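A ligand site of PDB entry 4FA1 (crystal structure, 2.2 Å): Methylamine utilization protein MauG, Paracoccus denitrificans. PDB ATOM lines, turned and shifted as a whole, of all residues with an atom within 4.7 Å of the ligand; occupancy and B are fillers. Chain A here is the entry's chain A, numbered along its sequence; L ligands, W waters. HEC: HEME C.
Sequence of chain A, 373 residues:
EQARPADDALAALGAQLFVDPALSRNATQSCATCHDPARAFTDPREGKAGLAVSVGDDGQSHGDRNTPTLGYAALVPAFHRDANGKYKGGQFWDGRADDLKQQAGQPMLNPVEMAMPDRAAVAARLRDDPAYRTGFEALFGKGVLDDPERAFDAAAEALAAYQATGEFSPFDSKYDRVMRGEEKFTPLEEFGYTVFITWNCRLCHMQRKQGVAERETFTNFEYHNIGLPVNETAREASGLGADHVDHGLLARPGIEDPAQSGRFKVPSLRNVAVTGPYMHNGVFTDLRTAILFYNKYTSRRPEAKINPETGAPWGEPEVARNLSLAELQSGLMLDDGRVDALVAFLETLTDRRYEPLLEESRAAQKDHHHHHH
The side-chain sulfur of Cys 31 is covalently linked to a carbon (CAB) of the ligand.
N of Phe 92 sits at hydrogen-bond distance from O2A of the ligand, at 2.6 Å.
A ring nitrogen (NE2) of His 35 is bound to an iron atom (FE) of the ligand, 2.1 Å away.
The backbone NH (N) of Trp 93 lies within hydrogen-bond range of an oxygen (O2D) of the ligand.
An oxygen (O1A) of the ligand lies within salt-bridge range of the side-chain amino group (NZ) of Lys 265.
The guanidinium group (NH2) of Arg 96 is in salt-bridge range of an oxygen (O1D) of the ligand (2.6 Å).
The side-chain sulfur of Cys 34 is covalently linked to a carbon (CAC) of the ligand (1.8 Å).
An oxygen (O1D) of the ligand lies within salt-bridge range of the guanidinium group (NH1) of Arg 65, 3.1 Å away.
Water W2 lies within hydrogen-bond range of the side-chain carboxylate of Glu 113 and the side-chain amide nitrogen of Gln 103.
Water W3 bridges O2A of the ligand (3.0 Å) and NZ of Lys 265 (3.3 Å).
Water W1 bridges N of Ser 54 (2.8 Å) and O of Arg 65 (2.9 Å).
A nitrogen (NA) of the ligand sits close to the side-chain amide nitrogen (NE2) of Gln 103 (3.1 Å).
Gln 29 touches the ligand.
O of Ser 30 touches CMC of the ligand, at 3.7 Å.
Ser 54 touches the ligand (CB to CAC, 3.7 Å).
Val 55 touches the ligand.
Asn 66 touches the ligand.
Thr 67 touches the ligand.
Pro 68 touches the ligand (CD to C3D, 3.3 Å).
Leu 70 touches the ligand.
Gln 91 touches the ligand.
CD2 of Leu 100 touches CMA of the ligand, at 3.2 Å.
Ala 104 touches the ligand (O to CBB, 3.3 Å).
Pro 107 touches the ligand (CB to CHC, 3.3 Å).
CE of Met 108 touches CBB of the ligand, 3.7 Å away.
Glu 113 touches the ligand.
Met 114 touches the ligand (CG to CMC, 3.5 Å).
Leu 159 touches the ligand (CD1 to CBB, 3.8 Å).
Gln 163 touches the ligand.
Hydrophobic or aromatic side chains that line the ligand: His 35, Pro 68, Leu 70, Phe 92, Trp 93, Leu 100, Pro 107, Met 108, Met 114 and Leu 159.
Of the 32 residues printed, 26 come within 4 Å of the ligand.
Along chain A the residues within 4 Å of the ligand span positions 29 to 265.
The nearest printed residue that does not touch the ligand is Gly 56 (4.01 Å).
O of Pro 68 is in hydrogen-bond range of ND1 of His 35 (3.0 Å).
The backbone carbonyl oxygen (O) of Phe 18 is in hydrogen-bond range of the backbone NH (N) of Cys 31, 3.2 Å away.
The side-chain amide nitrogen of Gln 29 lies close to the backbone carbonyl oxygen of Glu 113.
The backbone carbonyl oxygen of Pro 107 sits at hydrogen-bond distance from the backbone NH of Met 114 (3.1 Å).
OE1 of Gln 163 sits close to O of Leu 159, at 3.3 Å.
NH2 of Arg 96 is in salt-bridge range of OD2 of Asp 94 (2.8 Å).
N of Lys 265 lies within hydrogen-bond range of O of Trp 93.
The backbone NH (N) of Arg 96 sits at hydrogen-bond distance from the backbone carbonyl oxygen (O) of Gln 91 (3.3 Å).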
ATOM      1  N   PHE A  18     -17.524   6.604  23.548  1.00  0.00           N
ATOM      2  CA  PHE A  18     -16.855   6.283  22.294  1.00  0.00           C
ATOM      3  C   PHE A  18     -17.786   5.798  21.206  1.00  0.00           C
ATOM      4  O   PHE A  18     -17.552   6.110  20.017  1.00  0.00           O
ATOM      5  CB  PHE A  18     -15.819   5.190  22.511  1.00  0.00           C
ATOM      6  CG  PHE A  18     -14.898   4.992  21.348  1.00  0.00           C
ATOM      7  CD1 PHE A  18     -13.764   5.798  21.207  1.00  0.00           C
ATOM      8  CD2 PHE A  18     -15.123   4.002  20.402  1.00  0.00           C
ATOM      9  CE1 PHE A  18     -12.882   5.621  20.181  1.00  0.00           C
ATOM     10  CE2 PHE A  18     -14.264   3.849  19.333  1.00  0.00           C
ATOM     11  CZ  PHE A  18     -13.144   4.651  19.231  1.00  0.00           C
ATOM     12  N   GLN A  29     -23.466  10.103  14.278  1.00  0.00           N
ATOM     13  CA  GLN A  29     -22.124   9.511  14.361  1.00  0.00           C
ATOM     14  C   GLN A  29     -21.344   9.662  15.667  1.00  0.00           C
ATOM     15  O   GLN A  29     -21.455  10.670  16.373  1.00  0.00           O
ATOM     16  CB  GLN A  29     -21.270   9.903  13.142  1.00  0.00           C
ATOM     17  CG  GLN A  29     -20.594  11.267  13.190  1.00  0.00           C
ATOM     18  CD  GLN A  29     -19.554  11.456  12.085  1.00  0.00           C
ATOM     19  OE1 GLN A  29     -19.531  10.741  11.115  1.00  0.00           O
ATOM     20  NE2 GLN A  29     -18.726  12.430  12.253  1.00  0.00           N
ATOM     21  N   SER A  30     -20.561   8.630  15.974  1.00  0.00           N
ATOM     22  CA  SER A  30     -19.778   8.526  17.181  1.00  0.00           C
ATOM     23  C   SER A  30     -18.346   8.330  16.763  1.00  0.00           C
ATOM     24  O   SER A  30     -18.111   8.081  15.569  1.00  0.00           O
ATOM     25  CB  SER A  30     -20.213   7.316  17.974  1.00  0.00           C
ATOM     26  OG  SER A  30     -19.865   6.137  17.288  1.00  0.00           O
ATOM     27  N   CYS A  31     -17.404   8.399  17.732  1.00  0.00           N
ATOM     28  CA  CYS A  31     -15.975   8.163  17.439  1.00  0.00           C
ATOM     29  C   CYS A  31     -15.827   6.865  16.655  1.00  0.00           C
ATOM     30  O   CYS A  31     -15.025   6.790  15.718  1.00  0.00           O
ATOM     31  CB  CYS A  31     -15.119   7.997  18.694  1.00  0.00           C
ATOM     32  SG  CYS A  31     -15.322   9.198  20.008  1.00  0.00           S
ATOM     33  N   CYS A  34     -15.996   6.565  12.816  1.00  0.00           N
ATOM     34  CA  CYS A  34     -14.815   6.732  12.010  1.00  0.00           C
ATOM     35  C   CYS A  34     -13.709   5.837  12.470  1.00  0.00           C
ATOM     36  O   CYS A  34     -12.922   5.383  11.631  1.00  0.00           O
ATOM     37  CB  CYS A  34     -14.346   8.182  11.965  1.00  0.00           C
ATOM     38  SG  CYS A  34     -15.490   9.234  11.125  1.00  0.00           S
ATOM     39  N   HIS A  35     -13.634   5.593  13.768  1.00  0.00           N
ATOM     40  CA  HIS A  35     -12.606   4.757  14.313  1.00  0.00           C
ATOM     41  C   HIS A  35     -13.293   3.478  14.689  1.00  0.00           C
ATOM     42  O   HIS A  35     -13.534   3.180  15.867  1.00  0.00           O
ATOM     43  CB  HIS A  35     -11.942   5.435  15.514  1.00  0.00           C
ATOM     44  CG  HIS A  35     -11.255   6.724  15.186  1.00  0.00           C
ATOM     45  ND1 HIS A  35     -10.011   6.791  14.612  1.00  0.00           N
ATOM     46  CD2 HIS A  35     -11.638   8.011  15.392  1.00  0.00           C
ATOM     47  CE1 HIS A  35      -9.641   8.057  14.479  1.00  0.00           C
ATOM     48  NE2 HIS A  35     -10.617   8.819  14.960  1.00  0.00           N
ATOM     49  N   ARG A  45     -16.044   3.335   5.713  1.00  0.00           N
ATOM     50  CA  ARG A  45     -17.123   3.907   4.880  1.00  0.00           C
ATOM     51  C   ARG A  45     -16.579   4.607   3.635  1.00  0.00           C
ATOM     52  O   ARG A  45     -15.601   5.375   3.746  1.00  0.00           O
ATOM     53  CB  ARG A  45     -18.013   4.846   5.706  1.00  0.00           C
ATOM     54  CG  ARG A  45     -18.667   4.223   6.945  1.00  0.00           C
ATOM     55  CD  ARG A  45     -19.304   5.319   7.800  1.00  0.00           C
ATOM     56  NE  ARG A  45     -18.296   6.354   8.059  1.00  0.00           N
ATOM     57  CZ  ARG A  45     -18.573   7.642   8.255  1.00  0.00           C
ATOM     58  NH1 ARG A  45     -19.851   8.082   8.252  1.00  0.00           N
ATOM     59  NH2 ARG A  45     -17.577   8.496   8.447  1.00  0.00           N
ATOM     60  N   SER A  54     -12.768  10.687   5.538  1.00  0.00           N
ATOM     61  CA  SER A  54     -14.049  10.317   6.130  1.00  0.00           C
ATOM     62  C   SER A  54     -15.124  11.396   5.970  1.00  0.00           C
ATOM     63  O   SER A  54     -14.801  12.606   5.793  1.00  0.00           O
ATOM     64  CB  SER A  54     -13.822   9.997   7.618  1.00  0.00           C
ATOM     65  OG  SER A  54     -12.885   8.935   7.726  1.00  0.00           O
ATOM     66  N   VAL A  55     -16.404  10.962   6.049  1.00  0.00           N
ATOM     67  CA  VAL A  55     -17.555  11.876   6.019  1.00  0.00           C
ATOM     68  C   VAL A  55     -18.073  12.173   7.427  1.00  0.00           C
ATOM     69  O   VAL A  55     -18.319  11.267   8.217  1.00  0.00           O
ATOM     70  CB  VAL A  55     -18.736  11.349   5.148  1.00  0.00           C
ATOM     71  CG1 VAL A  55     -19.841  12.385   5.055  1.00  0.00           C
ATOM     72  CG2 VAL A  55     -18.265  10.983   3.766  1.00  0.00           C
ATOM     73  N   GLY A  56     -18.278  13.457   7.730  1.00  0.00           N
ATOM     74  CA  GLY A  56     -18.777  13.887   9.019  1.00  0.00           C
ATOM     75  C   GLY A  56     -20.263  13.630   9.290  1.00  0.00           C
ATOM     76  O   GLY A  56     -20.971  12.985   8.503  1.00  0.00           O
ATOM     77  N   ARG A  65      -7.719  14.511   5.446  1.00  0.00           N
ATOM     78  CA  ARG A  65      -6.748  13.542   5.910  1.00  0.00           C
ATOM     79  C   ARG A  65      -7.404  12.218   6.175  1.00  0.00           C
ATOM     80  O   ARG A  65      -8.589  12.145   6.517  1.00  0.00           O
ATOM     81  CB  ARG A  65      -6.027  14.049   7.169  1.00  0.00           C
ATOM     82  CG  ARG A  65      -4.950  15.043   6.853  1.00  0.00           C
ATOM     83  CD  ARG A  65      -4.362  15.599   8.099  1.00  0.00           C
ATOM     84  NE  ARG A  65      -3.531  16.759   7.814  1.00  0.00           N
ATOM     85  CZ  ARG A  65      -3.103  17.599   8.758  1.00  0.00           C
ATOM     86  NH1 ARG A  65      -3.446  17.407  10.028  1.00  0.00           N
ATOM     87  NH2 ARG A  65      -2.324  18.622   8.451  1.00  0.00           N
ATOM     88  N   ASN A  66      -6.617  11.168   6.010  1.00  0.00           N
ATOM     89  CA  ASN A  66      -7.017   9.802   6.293  1.00  0.00           C
ATOM     90  C   ASN A  66      -7.210   9.567   7.780  1.00  0.00           C
ATOM     91  O   ASN A  66      -6.393  10.025   8.592  1.00  0.00           O
ATOM     92  CB  ASN A  66      -5.969   8.848   5.783  1.00  0.00           C
ATOM     93  CG  ASN A  66      -6.410   7.431   5.871  1.00  0.00           C
ATOM     94  OD1 ASN A  66      -5.681   6.558   6.360  1.00  0.00           O
ATOM     95  ND2 ASN A  66      -7.645   7.191   5.447  1.00  0.00           N
ATOM     96  N   THR A  67      -8.273   8.842   8.118  1.00  0.00           N
ATOM     97  CA  THR A  67      -8.567   8.558   9.517  1.00  0.00           C
ATOM     98  C   THR A  67      -7.544   7.532  10.032  1.00  0.00           C
ATOM     99  O   THR A  67      -7.486   6.431   9.550  1.00  0.00           O
ATOM    100  CB  THR A  67     -10.044   8.119   9.673  1.00  0.00           C
ATOM    101  OG1 THR A  67     -10.891   9.248   9.440  1.00  0.00           O
ATOM    102  CG2 THR A  67     -10.341   7.515  11.065  1.00  0.00           C
ATOM    103  N   PRO A  68      -6.699   7.914  11.007  1.00  0.00           N
ATOM    104  CA  PRO A  68      -5.760   6.936  11.564  1.00  0.00           C
ATOM    105  C   PRO A  68      -6.342   5.962  12.641  1.00  0.00           C
ATOM    106  O   PRO A  68      -7.365   6.243  13.316  1.00  0.00           O
ATOM    107  CB  PRO A  68      -4.671   7.812  12.176  1.00  0.00           C
ATOM    108  CG  PRO A  68      -5.376   9.057  12.539  1.00  0.00           C
ATOM    109  CD  PRO A  68      -6.580   9.213  11.651  1.00  0.00           C
ATOM    110  N   THR A  69      -5.685   4.834  12.799  1.00  0.00           N
ATOM    111  CA  THR A  69      -5.998   3.914  13.870  1.00  0.00           C
ATOM    112  C   THR A  69      -5.789   4.591  15.237  1.00  0.00           C
ATOM    113  O   THR A  69      -4.936   5.482  15.389  1.00  0.00           O
ATOM    114  CB  THR A  69      -5.088   2.679  13.809  1.00  0.00           C
ATOM    115  OG1 THR A  69      -5.472   1.780  14.828  1.00  0.00           O
ATOM    116  CG2 THR A  69      -3.602   3.079  14.046  1.00  0.00           C
ATOM    117  N   LEU A  70      -6.568   4.145  16.222  1.00  0.00           N
ATOM    118  CA  LEU A  70      -6.382   4.577  17.603  1.00  0.00           C
ATOM    119  C   LEU A  70      -5.550   3.544  18.396  1.00  0.00           C
ATOM    120  O   LEU A  70      -5.156   3.789  19.537  1.00  0.00           O
ATOM    121  CB  LEU A  70      -7.753   4.785  18.275  1.00  0.00           C
ATOM    122  CG  LEU A  70      -8.694   5.814  17.627  1.00  0.00           C
ATOM    123  CD1 LEU A  70      -9.796   6.206  18.611  1.00  0.00           C
ATOM    124  CD2 LEU A  70      -7.934   7.050  17.137  1.00  0.00           C
ATOM    125  N   GLN A  91      -0.544  14.169  18.919  1.00  0.00           N
ATOM    126  CA  GLN A  91      -1.597  13.485  18.167  1.00  0.00           C
ATOM    127  C   GLN A  91      -2.061  14.300  16.948  1.00  0.00           C
ATOM    128  O   GLN A  91      -1.854  15.509  16.857  1.00  0.00           O
ATOM    129  CB  GLN A  91      -2.789  13.117  19.069  1.00  0.00           C
ATOM    130  CG  GLN A  91      -2.413  12.262  20.256  1.00  0.00           C
ATOM    131  CD  GLN A  91      -2.028  10.827  19.948  1.00  0.00           C
ATOM    132  OE1 GLN A  91      -1.340  10.179  20.781  1.00  0.00           O
ATOM    133  NE2 GLN A  91      -2.477  10.307  18.818  1.00  0.00           N
ATOM    134  N   PHE A  92      -2.716  13.591  16.046  1.00  0.00           N
ATOM    135  CA  PHE A  92      -3.025  14.046  14.674  1.00  0.00           C
ATOM    136  C   PHE A  92      -1.780  13.852  13.805  1.00  0.00           C
ATOM    137  O   PHE A  92      -0.695  13.756  14.307  1.00  0.00           O
ATOM    138  CB  PHE A  92      -3.514  15.496  14.618  1.00  0.00           C
ATOM    139  CG  PHE A  92      -4.917  15.726  15.180  1.00  0.00           C
ATOM    140  CD1 PHE A  92      -6.018  15.007  14.722  1.00  0.00           C
ATOM    141  CD2 PHE A  92      -5.118  16.714  16.138  1.00  0.00           C
ATOM    142  CE1 PHE A  92      -7.308  15.235  15.215  1.00  0.00           C
ATOM    143  CE2 PHE A  92      -6.392  16.973  16.625  1.00  0.00           C
ATOM    144  CZ  PHE A  92      -7.491  16.226  16.165  1.00  0.00           C
ATOM    145  N   TRP A  93      -1.979  13.775  12.502  1.00  0.00           N
ATOM    146  CA  TRP A  93      -0.894  13.636  11.539  1.00  0.00           C
ATOM    147  C   TRP A  93       0.098  14.796  11.554  1.00  0.00           C
ATOM    148  O   TRP A  93       1.222  14.658  11.034  1.00  0.00           O
ATOM    149  CB  TRP A  93      -1.472  13.533  10.155  1.00  0.00           C
ATOM    150  CG  TRP A  93      -2.131  12.217   9.796  1.00  0.00           C
ATOM    151  CD1 TRP A  93      -3.465  11.960   9.753  1.00  0.00           C
ATOM    152  CD2 TRP A  93      -1.481  11.017   9.351  1.00  0.00           C
ATOM    153  NE1 TRP A  93      -3.690  10.664   9.332  1.00  0.00           N
ATOM    154  CE2 TRP A  93      -2.483  10.078   9.056  1.00  0.00           C
ATOM    155  CE3 TRP A  93      -0.132  10.654   9.168  1.00  0.00           C
ATOM    156  CZ2 TRP A  93      -2.187   8.763   8.607  1.00  0.00           C
ATOM    157  CZ3 TRP A  93       0.161   9.345   8.714  1.00  0.00           C
ATOM    158  CH2 TRP A  93      -0.864   8.426   8.422  1.00  0.00           C
ATOM    159  N   ASP A  94      -0.340  15.923  12.106  1.00  0.00           N
ATOM    160  CA  ASP A  94       0.489  17.124  12.184  1.00  0.00           C
ATOM    161  C   ASP A  94       0.839  17.464  13.609  1.00  0.00           C
ATOM    162  O   ASP A  94       1.327  18.549  13.880  1.00  0.00           O
ATOM    163  CB  ASP A  94      -0.146  18.333  11.496  1.00  0.00           C
ATOM    164  CG  ASP A  94      -1.596  18.606  11.918  1.00  0.00           C
ATOM    165  OD1 ASP A  94      -2.257  19.417  11.206  1.00  0.00           O
ATOM    166  OD2 ASP A  94      -2.094  18.008  12.904  1.00  0.00           O
ATOM    167  N   ARG A  96      -0.735  18.525  15.944  1.00  0.00           N
ATOM    168  CA  ARG A  96      -1.403  19.701  16.490  1.00  0.00           C
ATOM    169  C   ARG A  96      -2.069  19.505  17.896  1.00  0.00           C
ATOM    170  O   ARG A  96      -2.367  20.473  18.594  1.00  0.00           O
ATOM    171  CB  ARG A  96      -2.362  20.304  15.469  1.00  0.00           C
ATOM    172  CG  ARG A  96      -3.684  19.577  15.272  1.00  0.00           C
ATOM    173  CD  ARG A  96      -4.629  20.371  14.349  1.00  0.00           C
ATOM    174  NE  ARG A  96      -5.896  19.683  13.994  1.00  0.00           N
ATOM    175  CZ  ARG A  96      -5.987  18.627  13.178  1.00  0.00           C
ATOM    176  NH1 ARG A  96      -7.170  18.088  12.894  1.00  0.00           N
ATOM    177  NH2 ARG A  96      -4.879  18.098  12.654  1.00  0.00           N
ATOM    178  N   LEU A 100      -3.674  12.552  23.923  1.00  0.00           N
ATOM    179  CA  LEU A 100      -5.004  11.980  23.651  1.00  0.00           C
ATOM    180  C   LEU A 100      -6.115  12.813  24.286  1.00  0.00           C
ATOM    181  O   LEU A 100      -7.196  12.994  23.716  1.00  0.00           O
ATOM    182  CB  LEU A 100      -5.060  10.562  24.161  1.00  0.00           C
ATOM    183  CG  LEU A 100      -4.385   9.535  23.283  1.00  0.00           C
ATOM    184  CD1 LEU A 100      -4.263   8.137  24.039  1.00  0.00           C
ATOM    185  CD2 LEU A 100      -5.160   9.439  21.906  1.00  0.00           C
ATOM    186  N   GLN A 103      -6.638  15.897  22.240  1.00  0.00           N
ATOM    187  CA  GLN A 103      -7.200  15.518  20.944  1.00  0.00           C
ATOM    188  C   GLN A 103      -8.680  15.227  21.031  1.00  0.00           C
ATOM    189  O   GLN A 103      -9.396  15.664  20.138  1.00  0.00           O
ATOM    190  CB  GLN A 103      -6.510  14.292  20.338  1.00  0.00           C
ATOM    191  CG  GLN A 103      -6.866  14.040  18.874  1.00  0.00           C
ATOM    192  CD  GLN A 103      -8.241  13.426  18.731  1.00  0.00           C
ATOM    193  OE1 GLN A 103      -8.771  12.815  19.669  1.00  0.00           O
ATOM    194  NE2 GLN A 103      -8.835  13.587  17.586  1.00  0.00           N
ATOM    195  N   ALA A 104      -9.125  14.513  22.080  1.00  0.00           N
ATOM    196  CA  ALA A 104     -10.458  13.878  22.143  1.00  0.00           C
ATOM    197  C   ALA A 104     -11.639  14.756  21.827  1.00  0.00           C
ATOM    198  O   ALA A 104     -12.599  14.298  21.254  1.00  0.00           O
ATOM    199  CB  ALA A 104     -10.698  13.096  23.499  1.00  0.00           C
ATOM    200  N   PRO A 107     -12.771  16.296  17.572  1.00  0.00           N
ATOM    201  CA  PRO A 107     -13.773  15.676  16.683  1.00  0.00           C
ATOM    202  C   PRO A 107     -15.228  16.115  16.990  1.00  0.00           C
ATOM    203  O   PRO A 107     -16.044  16.335  16.071  1.00  0.00           O
ATOM    204  CB  PRO A 107     -13.630  14.184  16.962  1.00  0.00           C
ATOM    205  CG  PRO A 107     -12.277  14.006  17.545  1.00  0.00           C
ATOM    206  CD  PRO A 107     -11.825  15.298  18.117  1.00  0.00           C
ATOM    207  N   MET A 108     -15.541  16.207  18.291  1.00  0.00           N
ATOM    208  CA  MET A 108     -16.870  16.580  18.732  1.00  0.00           C
ATOM    209  C   MET A 108     -17.308  17.927  18.240  1.00  0.00           C
ATOM    210  O   MET A 108     -18.489  18.128  18.031  1.00  0.00           O
ATOM    211  CB  MET A 108     -16.971  16.597  20.259  1.00  0.00           C
ATOM    212  CG  MET A 108     -16.988  15.216  20.862  1.00  0.00           C
ATOM    213  SD  MET A 108     -17.003  15.325  22.642  1.00  0.00           S
ATOM    214  CE  MET A 108     -15.764  14.110  23.031  1.00  0.00           C
ATOM    215  N   VAL A 112     -16.722  19.508  10.136  1.00  0.00           N
ATOM    216  CA  VAL A 112     -16.619  18.462   9.096  1.00  0.00           C
ATOM    217  C   VAL A 112     -16.634  17.040   9.696  1.00  0.00           C
ATOM    218  O   VAL A 112     -16.672  16.045   8.959  1.00  0.00           O
ATOM    219  CB  VAL A 112     -15.427  18.670   8.061  1.00  0.00           C
ATOM    220  CG1 VAL A 112     -15.178  20.162   7.769  1.00  0.00           C
ATOM    221  CG2 VAL A 112     -14.163  17.972   8.503  1.00  0.00           C
ATOM    222  N   GLU A 113     -16.668  16.935  11.028  1.00  0.00           N
ATOM    223  CA  GLU A 113     -16.797  15.639  11.720  1.00  0.00           C
ATOM    224  C   GLU A 113     -18.098  15.599  12.533  1.00  0.00           C
ATOM    225  O   GLU A 113     -19.201  15.648  11.983  1.00  0.00           O
ATOM    226  CB  GLU A 113     -15.530  15.328  12.563  1.00  0.00           C
ATOM    227  CG  GLU A 113     -14.228  15.323  11.693  1.00  0.00           C
ATOM    228  CD  GLU A 113     -12.900  15.051  12.462  1.00  0.00           C
ATOM    229  OE1 GLU A 113     -12.815  15.203  13.705  1.00  0.00           O
ATOM    230  OE2 GLU A 113     -11.915  14.652  11.799  1.00  0.00           O
ATOM    231  N   MET A 114     -17.985  15.556  13.839  1.00  0.00           N
ATOM    232  CA  MET A 114     -19.187  15.332  14.635  1.00  0.00           C
ATOM    233  C   MET A 114     -20.066  16.588  14.721  1.00  0.00           C
ATOM    234  O   MET A 114     -21.271  16.470  14.914  1.00  0.00           O
ATOM    235  CB  MET A 114     -18.871  14.695  15.980  1.00  0.00           C
ATOM    236  CG  MET A 114     -18.322  13.273  15.814  1.00  0.00           C
ATOM    237  SD  MET A 114     -17.444  12.582  17.235  1.00  0.00           S
ATOM    238  CE  MET A 114     -18.837  12.032  18.214  1.00  0.00           C
ATOM    239  N   LEU A 159     -12.519   9.524  27.326  1.00  0.00           N
ATOM    240  CA  LEU A 159     -12.113   8.998  26.006  1.00  0.00           C
ATOM    241  C   LEU A 159     -10.646   8.573  25.968  1.00  0.00           C
ATOM    242  O   LEU A 159     -10.321   7.444  25.530  1.00  0.00           O
ATOM    243  CB  LEU A 159     -12.457   9.944  24.862  1.00  0.00           C
ATOM    244  CG  LEU A 159     -13.986   9.881  24.632  1.00  0.00           C
ATOM    245  CD1 LEU A 159     -14.473  11.132  23.892  1.00  0.00           C
ATOM    246  CD2 LEU A 159     -14.382   8.588  23.869  1.00  0.00           C
ATOM    247  N   GLN A 163      -8.955   4.861  25.453  1.00  0.00           N
ATOM    248  CA  GLN A 163      -7.894   4.579  24.478  1.00  0.00           C
ATOM    249  C   GLN A 163      -6.535   4.137  25.084  1.00  0.00           C
ATOM    250  O   GLN A 163      -5.619   3.740  24.344  1.00  0.00           O
ATOM    251  CB  GLN A 163      -7.654   5.780  23.551  1.00  0.00           C
ATOM    252  CG  GLN A 163      -8.750   6.088  22.549  1.00  0.00           C
ATOM    253  CD  GLN A 163      -8.630   7.507  21.985  1.00  0.00           C
ATOM    254  OE1 GLN A 163      -8.941   8.482  22.681  1.00  0.00           O
ATOM    255  NE2 GLN A 163      -8.139   7.627  20.759  1.00  0.00           N
ATOM    256  N   LYS A 265       3.673  13.186  11.230  1.00  0.00           N
ATOM    257  CA  LYS A 265       4.076  12.267  12.269  1.00  0.00           C
ATOM    258  C   LYS A 265       4.268  10.890  11.702  1.00  0.00           C
ATOM    259  O   LYS A 265       3.423  10.435  10.927  1.00  0.00           O
ATOM    260  CB  LYS A 265       3.032  12.232  13.400  1.00  0.00           C
ATOM    261  CG  LYS A 265       3.270  11.157  14.477  1.00  0.00           C
ATOM    262  CD  LYS A 265       2.347  11.344  15.680  1.00  0.00           C
ATOM    263  CE  LYS A 265       0.814  11.108  15.403  1.00  0.00           C
ATOM    264  NZ  LYS A 265       0.442   9.816  14.715  1.00  0.00           N
HETATM  265 FE   HEC L   1     -10.701  10.883  15.128  1.00  0.00          FE
HETATM  266  CHA HEC L   1      -7.470  11.630  14.311  1.00  0.00           C
HETATM  267  CHB HEC L   1      -9.706   9.957  18.297  1.00  0.00           C
HETATM  268  CHC HEC L   1     -13.984  11.035  16.132  1.00  0.00           C
HETATM  269  CHD HEC L   1     -11.651  10.962  11.840  1.00  0.00           C
HETATM  270  NA  HEC L   1      -8.867  10.802  16.146  1.00  0.00           N
HETATM  271  C1A HEC L   1      -7.655  11.114  15.678  1.00  0.00           C
HETATM  272  C2A HEC L   1      -6.560  10.873  16.645  1.00  0.00           C
HETATM  273  C3A HEC L   1      -7.186  10.424  17.793  1.00  0.00           C
HETATM  274  C4A HEC L   1      -8.625  10.408  17.413  1.00  0.00           C
HETATM  275  CMA HEC L   1      -6.521  10.021  19.087  1.00  0.00           C
HETATM  276  CAA HEC L   1      -5.070  11.066  16.463  1.00  0.00           C
HETATM  277  CBA HEC L   1      -4.481   9.704  16.039  1.00  0.00           C
HETATM  278  CGA HEC L   1      -3.036   9.915  15.526  1.00  0.00           C
HETATM  279  O1A HEC L   1      -2.334   8.925  15.333  1.00  0.00           O
HETATM  280  O2A HEC L   1      -2.573  11.068  15.281  1.00  0.00           O
HETATM  281  NB  HEC L   1     -11.682  10.528  16.917  1.00  0.00           N
HETATM  282  C1B HEC L   1     -11.131  10.268  18.115  1.00  0.00           C
HETATM  283  C2B HEC L   1     -12.136  10.287  19.222  1.00  0.00           C
HETATM  284  C3B HEC L   1     -13.347  10.611  18.619  1.00  0.00           C
HETATM  285  C4B HEC L   1     -13.003  10.702  17.187  1.00  0.00           C
HETATM  286  CMB HEC L   1     -11.835  10.053  20.672  1.00  0.00           C
HETATM  287  CAB HEC L   1     -14.706  10.758  19.258  1.00  0.00           C
HETATM  288  CBB HEC L   1     -14.699  11.932  20.206  1.00  0.00           C
HETATM  289  NC  HEC L   1     -12.512  10.994  14.116  1.00  0.00           N
HETATM  290  C1C HEC L   1     -13.736  10.980  14.675  1.00  0.00           C
HETATM  291  C2C HEC L   1     -14.849  10.949  13.703  1.00  0.00           C
HETATM  292  C3C HEC L   1     -14.203  10.931  12.467  1.00  0.00           C
HETATM  293  C4C HEC L   1     -12.750  10.951  12.809  1.00  0.00           C
HETATM  294  CMC HEC L   1     -16.312  10.920  14.076  1.00  0.00           C
HETATM  295  CAC HEC L   1     -14.784  10.879  11.064  1.00  0.00           C
HETATM  296  CBC HEC L   1     -15.633  12.092  10.750  1.00  0.00           C
HETATM  297  ND  HEC L   1      -9.709  11.211  13.333  1.00  0.00           N
HETATM  298  C1D HEC L   1     -10.230  11.340  12.121  1.00  0.00           C
HETATM  299  C2D HEC L   1      -9.282  11.891  11.117  1.00  0.00           C
HETATM  300  C3D HEC L   1      -8.112  12.095  11.844  1.00  0.00           C
HETATM  301  C4D HEC L   1      -8.449  11.626  13.207  1.00  0.00           C
HETATM  302  CMD HEC L   1      -9.513  12.215   9.669  1.00  0.00           C
HETATM  303  CAD HEC L   1      -6.783  12.636  11.371  1.00  0.00           C
HETATM  304  CBD HEC L   1      -7.017  14.089  11.149  1.00  0.00           C
HETATM  305  CGD HEC L   1      -5.781  14.929  11.282  1.00  0.00           C
HETATM  306  O1D HEC L   1      -5.948  16.169  11.369  1.00  0.00           O
HETATM  307  O2D HEC L   1      -4.647  14.379  11.285  1.00  0.00           O
HETATM  308  O   HOH W   1     -11.377  12.583   7.053  1.00  0.00           O
HETATM  309  O   HOH W   2     -10.769  13.374  14.879  1.00  0.00           O
HETATM  310  O   HOH W   3      -2.017  10.034  12.573  1.00  0.00           O
